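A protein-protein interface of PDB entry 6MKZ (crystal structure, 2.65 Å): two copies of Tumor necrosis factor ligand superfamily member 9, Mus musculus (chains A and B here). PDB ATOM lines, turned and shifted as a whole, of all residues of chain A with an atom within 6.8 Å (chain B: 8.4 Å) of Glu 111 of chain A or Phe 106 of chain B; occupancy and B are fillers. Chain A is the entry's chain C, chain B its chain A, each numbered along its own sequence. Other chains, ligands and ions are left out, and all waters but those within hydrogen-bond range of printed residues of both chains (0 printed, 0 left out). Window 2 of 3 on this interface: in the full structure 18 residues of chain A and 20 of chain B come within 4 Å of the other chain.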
ATOM      1  N   PRO A  70     -17.429  11.375  17.123  1.00  0.00           N
ATOM      2  CA  PRO A  70     -16.994  11.363  15.718  1.00  0.00           C
ATOM      3  C   PRO A  70     -15.555  11.849  15.629  1.00  0.00           C
ATOM      4  O   PRO A  70     -15.103  12.625  16.481  1.00  0.00           O
ATOM      5  CB  PRO A  70     -17.985  12.297  15.027  1.00  0.00           C
ATOM      6  CG  PRO A  70     -18.459  13.214  16.081  1.00  0.00           C
ATOM      7  CD  PRO A  70     -18.349  12.509  17.395  1.00  0.00           C
ATOM      8  N   PHE A 106     -26.315   7.345  12.734  1.00  0.00           N
ATOM      9  CA  PHE A 106     -26.847   7.877  11.484  1.00  0.00           C
ATOM     10  C   PHE A 106     -25.952   8.978  10.958  1.00  0.00           C
ATOM     11  O   PHE A 106     -25.205   9.533  11.747  1.00  0.00           O
ATOM     12  CB  PHE A 106     -28.269   8.425  11.724  1.00  0.00           C
ATOM     13  CG  PHE A 106     -29.201   7.475  12.432  1.00  0.00           C
ATOM     14  CD1 PHE A 106     -29.774   6.404  11.754  1.00  0.00           C
ATOM     15  CD2 PHE A 106     -29.497   7.642  13.779  1.00  0.00           C
ATOM     16  CE1 PHE A 106     -30.636   5.525  12.407  1.00  0.00           C
ATOM     17  CE2 PHE A 106     -30.359   6.758  14.434  1.00  0.00           C
ATOM     18  CZ  PHE A 106     -30.929   5.711  13.740  1.00  0.00           C
ATOM     19  N   PRO A 107     -26.025   9.399   9.679  1.00  0.00           N
ATOM     20  CA  PRO A 107     -25.189  10.535   9.247  1.00  0.00           C
ATOM     21  C   PRO A 107     -25.382  11.787  10.124  1.00  0.00           C
ATOM     22  O   PRO A 107     -24.461  12.599  10.252  1.00  0.00           O
ATOM     23  CB  PRO A 107     -25.661  10.783   7.821  1.00  0.00           C
ATOM     24  CG  PRO A 107     -26.219   9.473   7.377  1.00  0.00           C
ATOM     25  CD  PRO A 107     -26.873   8.906   8.571  1.00  0.00           C
ATOM     26  N   CYS A 108     -26.563  11.906  10.765  1.00  0.00           N
ATOM     27  CA  CYS A 108     -26.969  13.001  11.648  1.00  0.00           C
ATOM     28  C   CYS A 108     -26.167  12.995  12.944  1.00  0.00           C
ATOM     29  O   CYS A 108     -25.884  14.054  13.509  1.00  0.00           O
ATOM     30  CB  CYS A 108     -28.465  12.899  11.941  1.00  0.00           C
ATOM     31  SG  CYS A 108     -29.067  14.058  13.200  1.00  0.00           S
ATOM     32  N   SER A 109     -25.819  11.801  13.414  1.00  0.00           N
ATOM     33  CA  SER A 109     -25.156  11.562  14.681  1.00  0.00           C
ATOM     34  C   SER A 109     -23.832  12.317  14.837  1.00  0.00           C
ATOM     35  O   SER A 109     -23.480  12.665  15.964  1.00  0.00           O
ATOM     36  CB  SER A 109     -24.929  10.072  14.884  1.00  0.00           C
ATOM     37  OG  SER A 109     -26.122   9.331  14.693  1.00  0.00           O
ATOM     38  N   MET A 110     -23.123  12.591  13.720  1.00  0.00           N
ATOM     39  CA  MET A 110     -21.845  13.311  13.659  1.00  0.00           C
ATOM     40  C   MET A 110     -21.966  14.751  14.173  1.00  0.00           C
ATOM     41  O   MET A 110     -20.936  15.370  14.436  1.00  0.00           O
ATOM     42  CB  MET A 110     -21.302  13.335  12.222  1.00  0.00           C
ATOM     43  CG  MET A 110     -21.421  12.022  11.498  1.00  0.00           C
ATOM     44  SD  MET A 110     -19.828  11.234  11.248  1.00  0.00           S
ATOM     45  CE  MET A 110     -20.169  10.364   9.768  1.00  0.00           C
ATOM     46  N   GLU A 111     -23.211  15.278  14.329  1.00  0.00           N
ATOM     47  CA  GLU A 111     -23.485  16.634  14.825  1.00  0.00           C
ATOM     48  C   GLU A 111     -23.292  16.725  16.346  1.00  0.00           C
ATOM     49  O   GLU A 111     -23.158  17.822  16.891  1.00  0.00           O
ATOM     50  CB  GLU A 111     -24.909  17.092  14.435  1.00  0.00           C
ATOM     51  N   ASN A 112     -23.261  15.569  17.017  1.00  0.00           N
ATOM     52  CA  ASN A 112     -23.048  15.439  18.451  1.00  0.00           C
ATOM     53  C   ASN A 112     -21.571  15.211  18.782  1.00  0.00           C
ATOM     54  O   ASN A 112     -20.955  14.311  18.211  1.00  0.00           O
ATOM     55  CB  ASN A 112     -23.867  14.257  18.982  1.00  0.00           C
ATOM     56  CG  ASN A 112     -25.243  14.617  19.397  1.00  0.00           C
ATOM     57  OD1 ASN A 112     -25.461  15.164  20.481  1.00  0.00           O
ATOM     58  ND2 ASN A 112     -26.188  14.315  18.538  1.00  0.00           N
ATOM     59  N   LYS A 113     -21.023  15.983  19.743  1.00  0.00           N
ATOM     60  CA  LYS A 113     -19.644  15.840  20.234  1.00  0.00           C
ATOM     61  C   LYS A 113     -19.485  14.498  20.946  1.00  0.00           C
ATOM     62  O   LYS A 113     -18.408  13.897  20.912  1.00  0.00           O
ATOM     63  CB  LYS A 113     -19.262  17.000  21.171  1.00  0.00           C
ATOM     64  CG  LYS A 113     -19.067  18.323  20.451  1.00  0.00           C
ATOM     65  CD  LYS A 113     -18.806  19.452  21.418  1.00  0.00           C
ATOM     66  CE  LYS A 113     -18.535  20.749  20.697  1.00  0.00           C
ATOM     67  NZ  LYS A 113     -18.100  21.814  21.640  1.00  0.00           N
ATOM     68  N   LEU A 114     -20.573  14.025  21.576  1.00  0.00           N
ATOM     69  CA  LEU A 114     -20.632  12.753  22.293  1.00  0.00           C
ATOM     70  C   LEU A 114     -21.992  12.062  22.087  1.00  0.00           C
ATOM     71  O   LEU A 114     -23.038  12.685  22.239  1.00  0.00           O
ATOM     72  CB  LEU A 114     -20.356  12.970  23.798  1.00  0.00           C
ATOM     73  CG  LEU A 114     -20.545  11.748  24.712  1.00  0.00           C
ATOM     74  CD1 LEU A 114     -19.252  11.080  24.998  1.00  0.00           C
ATOM     75  CD2 LEU A 114     -21.212  12.138  26.015  1.00  0.00           C
ATOM     76  N   TRP A 149     -15.777   6.878  13.728  1.00  0.00           N
ATOM     77  CA  TRP A 149     -16.241   6.877  15.120  1.00  0.00           C
ATOM     78  C   TRP A 149     -15.218   6.200  16.004  1.00  0.00           C
ATOM     79  O   TRP A 149     -14.524   5.263  15.593  1.00  0.00           O
ATOM     80  CB  TRP A 149     -17.621   6.210  15.306  1.00  0.00           C
ATOM     81  CG  TRP A 149     -18.760   7.047  14.800  1.00  0.00           C
ATOM     82  CD1 TRP A 149     -19.223   7.114  13.518  1.00  0.00           C
ATOM     83  CD2 TRP A 149     -19.512   8.015  15.550  1.00  0.00           C
ATOM     84  NE1 TRP A 149     -20.216   8.060  13.422  1.00  0.00           N
ATOM     85  CE2 TRP A 149     -20.439   8.604  14.660  1.00  0.00           C
ATOM     86  CE3 TRP A 149     -19.487   8.451  16.886  1.00  0.00           C
ATOM     87  CZ2 TRP A 149     -21.356   9.582  15.074  1.00  0.00           C
ATOM     88  CZ3 TRP A 149     -20.379   9.438  17.283  1.00  0.00           C
ATOM     89  CH2 TRP A 149     -21.288  10.001  16.381  1.00  0.00           C
ATOM     90  N   HIS B  77     -39.715  20.961   8.693  1.00  0.00           N
ATOM     91  CA  HIS B  77     -39.586  22.019   9.692  1.00  0.00           C
ATOM     92  C   HIS B  77     -38.555  21.656  10.761  1.00  0.00           C
ATOM     93  O   HIS B  77     -38.773  20.778  11.602  1.00  0.00           O
ATOM     94  CB  HIS B  77     -40.947  22.378  10.281  1.00  0.00           C
ATOM     95  CG  HIS B  77     -41.626  23.426   9.456  1.00  0.00           C
ATOM     96  ND1 HIS B  77     -42.439  23.087   8.390  1.00  0.00           N
ATOM     97  CD2 HIS B  77     -41.498  24.773   9.495  1.00  0.00           C
ATOM     98  CE1 HIS B  77     -42.821  24.234   7.849  1.00  0.00           C
ATOM     99  NE2 HIS B  77     -42.278  25.276   8.478  1.00  0.00           N
ATOM    100  N   LYS B  78     -37.413  22.359  10.685  1.00  0.00           N
ATOM    101  CA  LYS B  78     -36.225  22.208  11.514  1.00  0.00           C
ATOM    102  C   LYS B  78     -36.491  22.589  12.972  1.00  0.00           C
ATOM    103  O   LYS B  78     -36.822  23.737  13.266  1.00  0.00           O
ATOM    104  CB  LYS B  78     -35.087  23.057  10.929  1.00  0.00           C
ATOM    105  N   VAL B  79     -36.345  21.603  13.877  1.00  0.00           N
ATOM    106  CA  VAL B  79     -36.547  21.752  15.323  1.00  0.00           C
ATOM    107  C   VAL B  79     -35.213  21.578  16.048  1.00  0.00           C
ATOM    108  O   VAL B  79     -34.579  20.532  15.939  1.00  0.00           O
ATOM    109  CB  VAL B  79     -37.614  20.772  15.877  1.00  0.00           C
ATOM    110  CG1 VAL B  79     -37.905  21.043  17.351  1.00  0.00           C
ATOM    111  CG2 VAL B  79     -38.896  20.834  15.054  1.00  0.00           C
ATOM    112  N   GLN B  80     -34.806  22.598  16.800  1.00  0.00           N
ATOM    113  CA  GLN B  80     -33.564  22.546  17.556  1.00  0.00           C
ATOM    114  C   GLN B  80     -33.805  22.966  19.006  1.00  0.00           C
ATOM    115  O   GLN B  80     -34.840  23.565  19.310  1.00  0.00           O
ATOM    116  CB  GLN B  80     -32.474  23.407  16.893  1.00  0.00           C
ATOM    117  CG  GLN B  80     -32.906  24.818  16.492  1.00  0.00           C
ATOM    118  CD  GLN B  80     -31.829  25.630  15.794  1.00  0.00           C
ATOM    119  OE1 GLN B  80     -32.121  26.520  14.983  1.00  0.00           O
ATOM    120  NE2 GLN B  80     -30.558  25.363  16.091  1.00  0.00           N
ATOM    121  N   GLY B  81     -32.861  22.628  19.883  1.00  0.00           N
ATOM    122  CA  GLY B  81     -32.917  23.004  21.287  1.00  0.00           C
ATOM    123  C   GLY B  81     -32.190  22.075  22.233  1.00  0.00           C
ATOM    124  O   GLY B  81     -31.232  21.394  21.853  1.00  0.00           O
ATOM    125  N   TRP B  82     -32.642  22.061  23.489  1.00  0.00           N
ATOM    126  CA  TRP B  82     -32.081  21.214  24.525  1.00  0.00           C
ATOM    127  C   TRP B  82     -33.141  20.824  25.557  1.00  0.00           C
ATOM    128  O   TRP B  82     -34.119  21.548  25.771  1.00  0.00           O
ATOM    129  CB  TRP B  82     -30.868  21.886  25.223  1.00  0.00           C
ATOM    130  CG  TRP B  82     -31.184  23.214  25.856  1.00  0.00           C
ATOM    131  CD1 TRP B  82     -31.001  24.446  25.302  1.00  0.00           C
ATOM    132  CD2 TRP B  82     -31.802  23.437  27.136  1.00  0.00           C
ATOM    133  NE1 TRP B  82     -31.464  25.423  26.154  1.00  0.00           N
ATOM    134  CE2 TRP B  82     -31.957  24.831  27.289  1.00  0.00           C
ATOM    135  CE3 TRP B  82     -32.226  22.593  28.180  1.00  0.00           C
ATOM    136  CZ2 TRP B  82     -32.531  25.398  28.434  1.00  0.00           C
ATOM    137  CZ3 TRP B  82     -32.816  23.159  29.300  1.00  0.00           C
ATOM    138  CH2 TRP B  82     -32.937  24.546  29.431  1.00  0.00           C
ATOM    139  N   VAL B 103     -29.173  17.277  27.114  1.00  0.00           N
ATOM    140  CA  VAL B 103     -29.231  16.733  25.759  1.00  0.00           C
ATOM    141  C   VAL B 103     -29.518  17.853  24.774  1.00  0.00           C
ATOM    142  O   VAL B 103     -30.500  18.570  24.957  1.00  0.00           O
ATOM    143  CB  VAL B 103     -30.317  15.643  25.635  1.00  0.00           C
ATOM    144  CG1 VAL B 103     -30.277  14.986  24.266  1.00  0.00           C
ATOM    145  CG2 VAL B 103     -30.179  14.604  26.723  1.00  0.00           C
ATOM    146  N   GLU B 104     -28.700  17.975  23.717  1.00  0.00           N
ATOM    147  CA  GLU B 104     -28.922  18.931  22.633  1.00  0.00           C
ATOM    148  C   GLU B 104     -29.674  18.205  21.495  1.00  0.00           C
ATOM    149  O   GLU B 104     -29.332  17.065  21.142  1.00  0.00           O
ATOM    150  CB  GLU B 104     -27.597  19.545  22.138  1.00  0.00           C
ATOM    151  N   LEU B 105     -30.725  18.847  20.962  1.00  0.00           N
ATOM    152  CA  LEU B 105     -31.522  18.293  19.867  1.00  0.00           C
ATOM    153  C   LEU B 105     -31.349  19.146  18.634  1.00  0.00           C
ATOM    154  O   LEU B 105     -31.323  20.377  18.723  1.00  0.00           O
ATOM    155  CB  LEU B 105     -33.007  18.152  20.230  1.00  0.00           C
ATOM    156  CG  LEU B 105     -33.324  17.221  21.390  1.00  0.00           C
ATOM    157  CD1 LEU B 105     -34.611  17.600  22.035  1.00  0.00           C
ATOM    158  CD2 LEU B 105     -33.337  15.771  20.947  1.00  0.00           C
ATOM    159  N   PHE B 106     -31.198  18.483  17.488  1.00  0.00           N
ATOM    160  CA  PHE B 106     -30.962  19.115  16.191  1.00  0.00           C
ATOM    161  C   PHE B 106     -32.068  18.748  15.206  1.00  0.00           C
ATOM    162  O   PHE B 106     -32.753  17.737  15.422  1.00  0.00           O
ATOM    163  CB  PHE B 106     -29.590  18.675  15.640  1.00  0.00           C
ATOM    164  CG  PHE B 106     -28.453  18.829  16.617  1.00  0.00           C
ATOM    165  CD1 PHE B 106     -27.896  20.077  16.868  1.00  0.00           C
ATOM    166  CD2 PHE B 106     -27.933  17.727  17.281  1.00  0.00           C
ATOM    167  CE1 PHE B 106     -26.833  20.220  17.762  1.00  0.00           C
ATOM    168  CE2 PHE B 106     -26.873  17.870  18.181  1.00  0.00           C
ATOM    169  CZ  PHE B 106     -26.322  19.115  18.404  1.00  0.00           C
ATOM    170  N   PRO B 107     -32.245  19.554  14.124  1.00  0.00           N
ATOM    171  CA  PRO B 107     -33.309  19.275  13.139  1.00  0.00           C
ATOM    172  C   PRO B 107     -33.375  17.841  12.613  1.00  0.00           C
ATOM    173  O   PRO B 107     -34.466  17.387  12.253  1.00  0.00           O
ATOM    174  CB  PRO B 107     -32.970  20.223  11.997  1.00  0.00           C
ATOM    175  CG  PRO B 107     -32.324  21.366  12.657  1.00  0.00           C
ATOM    176  CD  PRO B 107     -31.517  20.794  13.768  1.00  0.00           C
ATOM    177  N   CYS B 108     -32.232  17.132  12.578  1.00  0.00           N
ATOM    178  CA  CYS B 108     -32.169  15.768  12.078  1.00  0.00           C
ATOM    179  C   CYS B 108     -32.308  14.738  13.204  1.00  0.00           C
ATOM    180  O   CYS B 108     -32.515  13.572  12.868  1.00  0.00           O
ATOM    181  CB  CYS B 108     -30.908  15.536  11.248  1.00  0.00           C
ATOM    182  SG  CYS B 108     -29.354  15.787  12.155  1.00  0.00           S
ATOM    183  N   SER B 109     -32.229  15.142  14.528  1.00  0.00           N
ATOM    184  CA  SER B 109     -32.419  14.233  15.693  1.00  0.00           C
ATOM    185  C   SER B 109     -33.730  13.449  15.580  1.00  0.00           C
ATOM    186  O   SER B 109     -33.830  12.350  16.130  1.00  0.00           O
ATOM    187  CB  SER B 109     -32.409  14.991  17.021  1.00  0.00           C
ATOM    188  OG  SER B 109     -31.209  15.707  17.236  1.00  0.00           O
ATOM    189  N   MET B 110     -34.710  14.003  14.836  1.00  0.00           N
ATOM    190  CA  MET B 110     -36.026  13.410  14.563  1.00  0.00           C
ATOM    191  C   MET B 110     -35.928  12.070  13.799  1.00  0.00           C
ATOM    192  O   MET B 110     -36.913  11.337  13.742  1.00  0.00           O
ATOM    193  CB  MET B 110     -36.901  14.395  13.772  1.00  0.00           C
ATOM    194  N   GLU B 111     -34.745  11.751  13.226  1.00  0.00           N
ATOM    195  CA  GLU B 111     -34.489  10.501  12.496  1.00  0.00           C
ATOM    196  C   GLU B 111     -34.295   9.317  13.472  1.00  0.00           C
ATOM    197  O   GLU B 111     -34.380   8.158  13.056  1.00  0.00           O
ATOM    198  CB  GLU B 111     -33.262  10.639  11.568  1.00  0.00           C
ATOM    199  CG  GLU B 111     -33.482  11.541  10.359  1.00  0.00           C
ATOM    200  CD  GLU B 111     -34.491  11.099   9.310  1.00  0.00           C
ATOM    201  OE1 GLU B 111     -34.693   9.873   9.141  1.00  0.00           O
ATOM    202  OE2 GLU B 111     -35.072  11.985   8.641  1.00  0.00           O
ATOM    203  N   ASN B 112     -34.038   9.622  14.758  1.00  0.00           N
ATOM    204  CA  ASN B 112     -33.849   8.648  15.831  1.00  0.00           C
ATOM    205  C   ASN B 112     -35.171   8.363  16.547  1.00  0.00           C
ATOM    206  O   ASN B 112     -35.848   9.301  16.967  1.00  0.00           O
ATOM    207  CB  ASN B 112     -32.813   9.159  16.840  1.00  0.00           C
ATOM    208  N   VAL B 115     -33.722   9.233  21.646  1.00  0.00           N
ATOM    209  CA  VAL B 115     -32.544  10.034  21.956  1.00  0.00           C
ATOM    210  C   VAL B 115     -32.331   9.863  23.485  1.00  0.00           C
ATOM    211  O   VAL B 115     -33.140  10.344  24.283  1.00  0.00           O
ATOM    212  CB  VAL B 115     -32.670  11.503  21.482  1.00  0.00           C
ATOM    213  CG1 VAL B 115     -31.544  12.352  22.047  1.00  0.00           C
ATOM    214  CG2 VAL B 115     -32.694  11.595  19.960  1.00  0.00           C
ATOM    215  N   ARG B 117     -29.472   9.732  26.937  1.00  0.00           N
ATOM    216  CA  ARG B 117     -28.275  10.290  27.581  1.00  0.00           C
ATOM    217  C   ARG B 117     -28.325  10.065  29.094  1.00  0.00           C
ATOM    218  O   ARG B 117     -29.357  10.267  29.724  1.00  0.00           O
ATOM    219  CB  ARG B 117     -28.059  11.774  27.265  1.00  0.00           C
ATOM    220  CG  ARG B 117     -26.787  12.334  27.913  1.00  0.00           C
ATOM    221  CD  ARG B 117     -26.357  13.634  27.316  1.00  0.00           C
ATOM    222  NE  ARG B 117     -25.622  13.412  26.088  1.00  0.00           N
ATOM    223  CZ  ARG B 117     -24.533  14.086  25.748  1.00  0.00           C
ATOM    224  NH1 ARG B 117     -24.043  15.025  26.551  1.00  0.00           N
ATOM    225  NH2 ARG B 117     -23.897  13.797  24.629  1.00  0.00           N
ATOM    226  N   LEU B 139     -37.114  24.541  23.391  1.00  0.00           N
ATOM    227  CA  LEU B 139     -37.196  24.121  22.007  1.00  0.00           C
ATOM    228  C   LEU B 139     -37.747  25.253  21.156  1.00  0.00           C
ATOM    229  O   LEU B 139     -38.662  25.966  21.567  1.00  0.00           O
ATOM    230  CB  LEU B 139     -38.037  22.843  21.878  1.00  0.00           C
ATOM    231  CG  LEU B 139     -37.437  21.599  22.563  1.00  0.00           C
ATOM    232  CD1 LEU B 139     -38.513  20.662  23.036  1.00  0.00           C
ATOM    233  CD2 LEU B 139     -36.426  20.889  21.669  1.00  0.00           C
ATOM    234  N   HIS B 140     -37.134  25.435  19.984  1.00  0.00           N
ATOM    235  CA  HIS B 140     -37.428  26.483  19.016  1.00  0.00           C
ATOM    236  C   HIS B 140     -37.238  25.936  17.603  1.00  0.00           C
ATOM    237  O   HIS B 140     -36.739  24.821  17.437  1.00  0.00           O
ATOM    238  CB  HIS B 140     -36.529  27.711  19.284  1.00  0.00           C
ATOM    239  CG  HIS B 140     -35.053  27.449  19.201  1.00  0.00           C
ATOM    240  ND1 HIS B 140     -34.258  28.202  18.358  1.00  0.00           N
ATOM    241  CD2 HIS B 140     -34.266  26.563  19.857  1.00  0.00           C
ATOM    242  CE1 HIS B 140     -33.030  27.742  18.508  1.00  0.00           C
ATOM    243  NE2 HIS B 140     -32.986  26.748  19.382  1.00  0.00           N
ATOM    244  N   TRP B 149     -41.207  16.988  20.657  1.00  0.00           N
ATOM    245  CA  TRP B 149     -40.460  16.012  21.459  1.00  0.00           C
ATOM    246  C   TRP B 149     -41.198  15.724  22.740  1.00  0.00           C
ATOM    247  O   TRP B 149     -41.885  16.586  23.300  1.00  0.00           O
ATOM    248  CB  TRP B 149     -39.020  16.458  21.774  1.00  0.00           C
ATOM    249  CG  TRP B 149     -38.103  16.387  20.593  1.00  0.00           C
ATOM    250  CD1 TRP B 149     -37.937  17.337  19.627  1.00  0.00           C
ATOM    251  CD2 TRP B 149     -37.292  15.275  20.206  1.00  0.00           C
ATOM    252  NE1 TRP B 149     -37.073  16.886  18.662  1.00  0.00           N
ATOM    253  CE2 TRP B 149     -36.644  15.630  19.002  1.00  0.00           C
ATOM    254  CE3 TRP B 149     -37.052  14.007  20.755  1.00  0.00           C
ATOM    255  CZ2 TRP B 149     -35.766  14.769  18.344  1.00  0.00           C
ATOM    256  CZ3 TRP B 149     -36.183  13.152  20.098  1.00  0.00           C
ATOM    257  CH2 TRP B 149     -35.563  13.529  18.898  1.00  0.00           C
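The side-chain sulfur of Cys 108 of chain A forms a disulfide with the side-chain sulfur of Cys 108 of chain B (2.0 Å). The backbone NH (N) of Ser 109 of chain B sits at hydrogen-bond distance from the side-chain sulfur (SG) of Cys 108 of chain A, at 3.6 Å. NH2 of Arg 117 of chain B sits at hydrogen-bond distance from O of Leu 114 of chain A (2.8 Å).
Among the printed residues, 5 pairs touch across the chains.
Of chain B, only Phe 106 comes within 4 Å of Glu 111 of chain A. Of the printed residues of chain A, Phe 106 of chain B touches Glu 111 (3.7 Å) and Asn 112 (3.6 Å). Asn 112 of chain A touches one residue of chain B. Printed residues of chain B within 4 Å of Cys 108 of chain A: Cys 108 and Ser 109. Of the printed residues of chain A, Ser 109 of chain B touches Cys 108 (3.6 Å). Of the printed residues of chain A, Cys 108 of chain B touches Cys 108 (2.0 Å). Of the printed residues of chain B, Leu 114 of chain A touches Arg 117 (2.8 Å). Of the printed residues of chain A, Arg 117 of chain B touches Leu 114. The nearest residue of chain A that does not touch Phe 106 of chain B is Cys 108 of chain A (5.2 Å). The nearest printed residue of chain B that does not touch Cys 108 of chain A is Phe 106 of chain B (5.2 Å).
The backbone NH (N) of Phe 106 of chain B sits at hydrogen-bond distance from the side-chain hydroxyl (OG) of Ser 109 of chain B, 2.8 Å away.
Among the printed residues, merely in contact across the chains: Asn 112 of chain A with Phe 106 of chain B (3.6 Å) and Glu 111 of chain A with Phe 106 of chain B (3.7 Å).
Cys 108 of chain A touches its own counterpart, Cys 108 of chain B. Cys 108 of chain A touches Ser 109 of chain B, but with the chains exchanged Ser 109 of chain A does not touch Cys 108 of chain B (5.5 Å). Glu 111 of chain A touches Phe 106 of chain B, but with the chains exchanged Phe 106 of chain A does not touch Glu 111 of chain B (4.3 Å). Asn 112 of chain A touches Phe 106 of chain B, but with the chains exchanged Phe 106 of chain A does not touch Asn 112 of chain B (4.2 Å). Of the 5 pairs that touch across the chains among the printed residues, 1 has its exchanged pair printed and touching as well.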
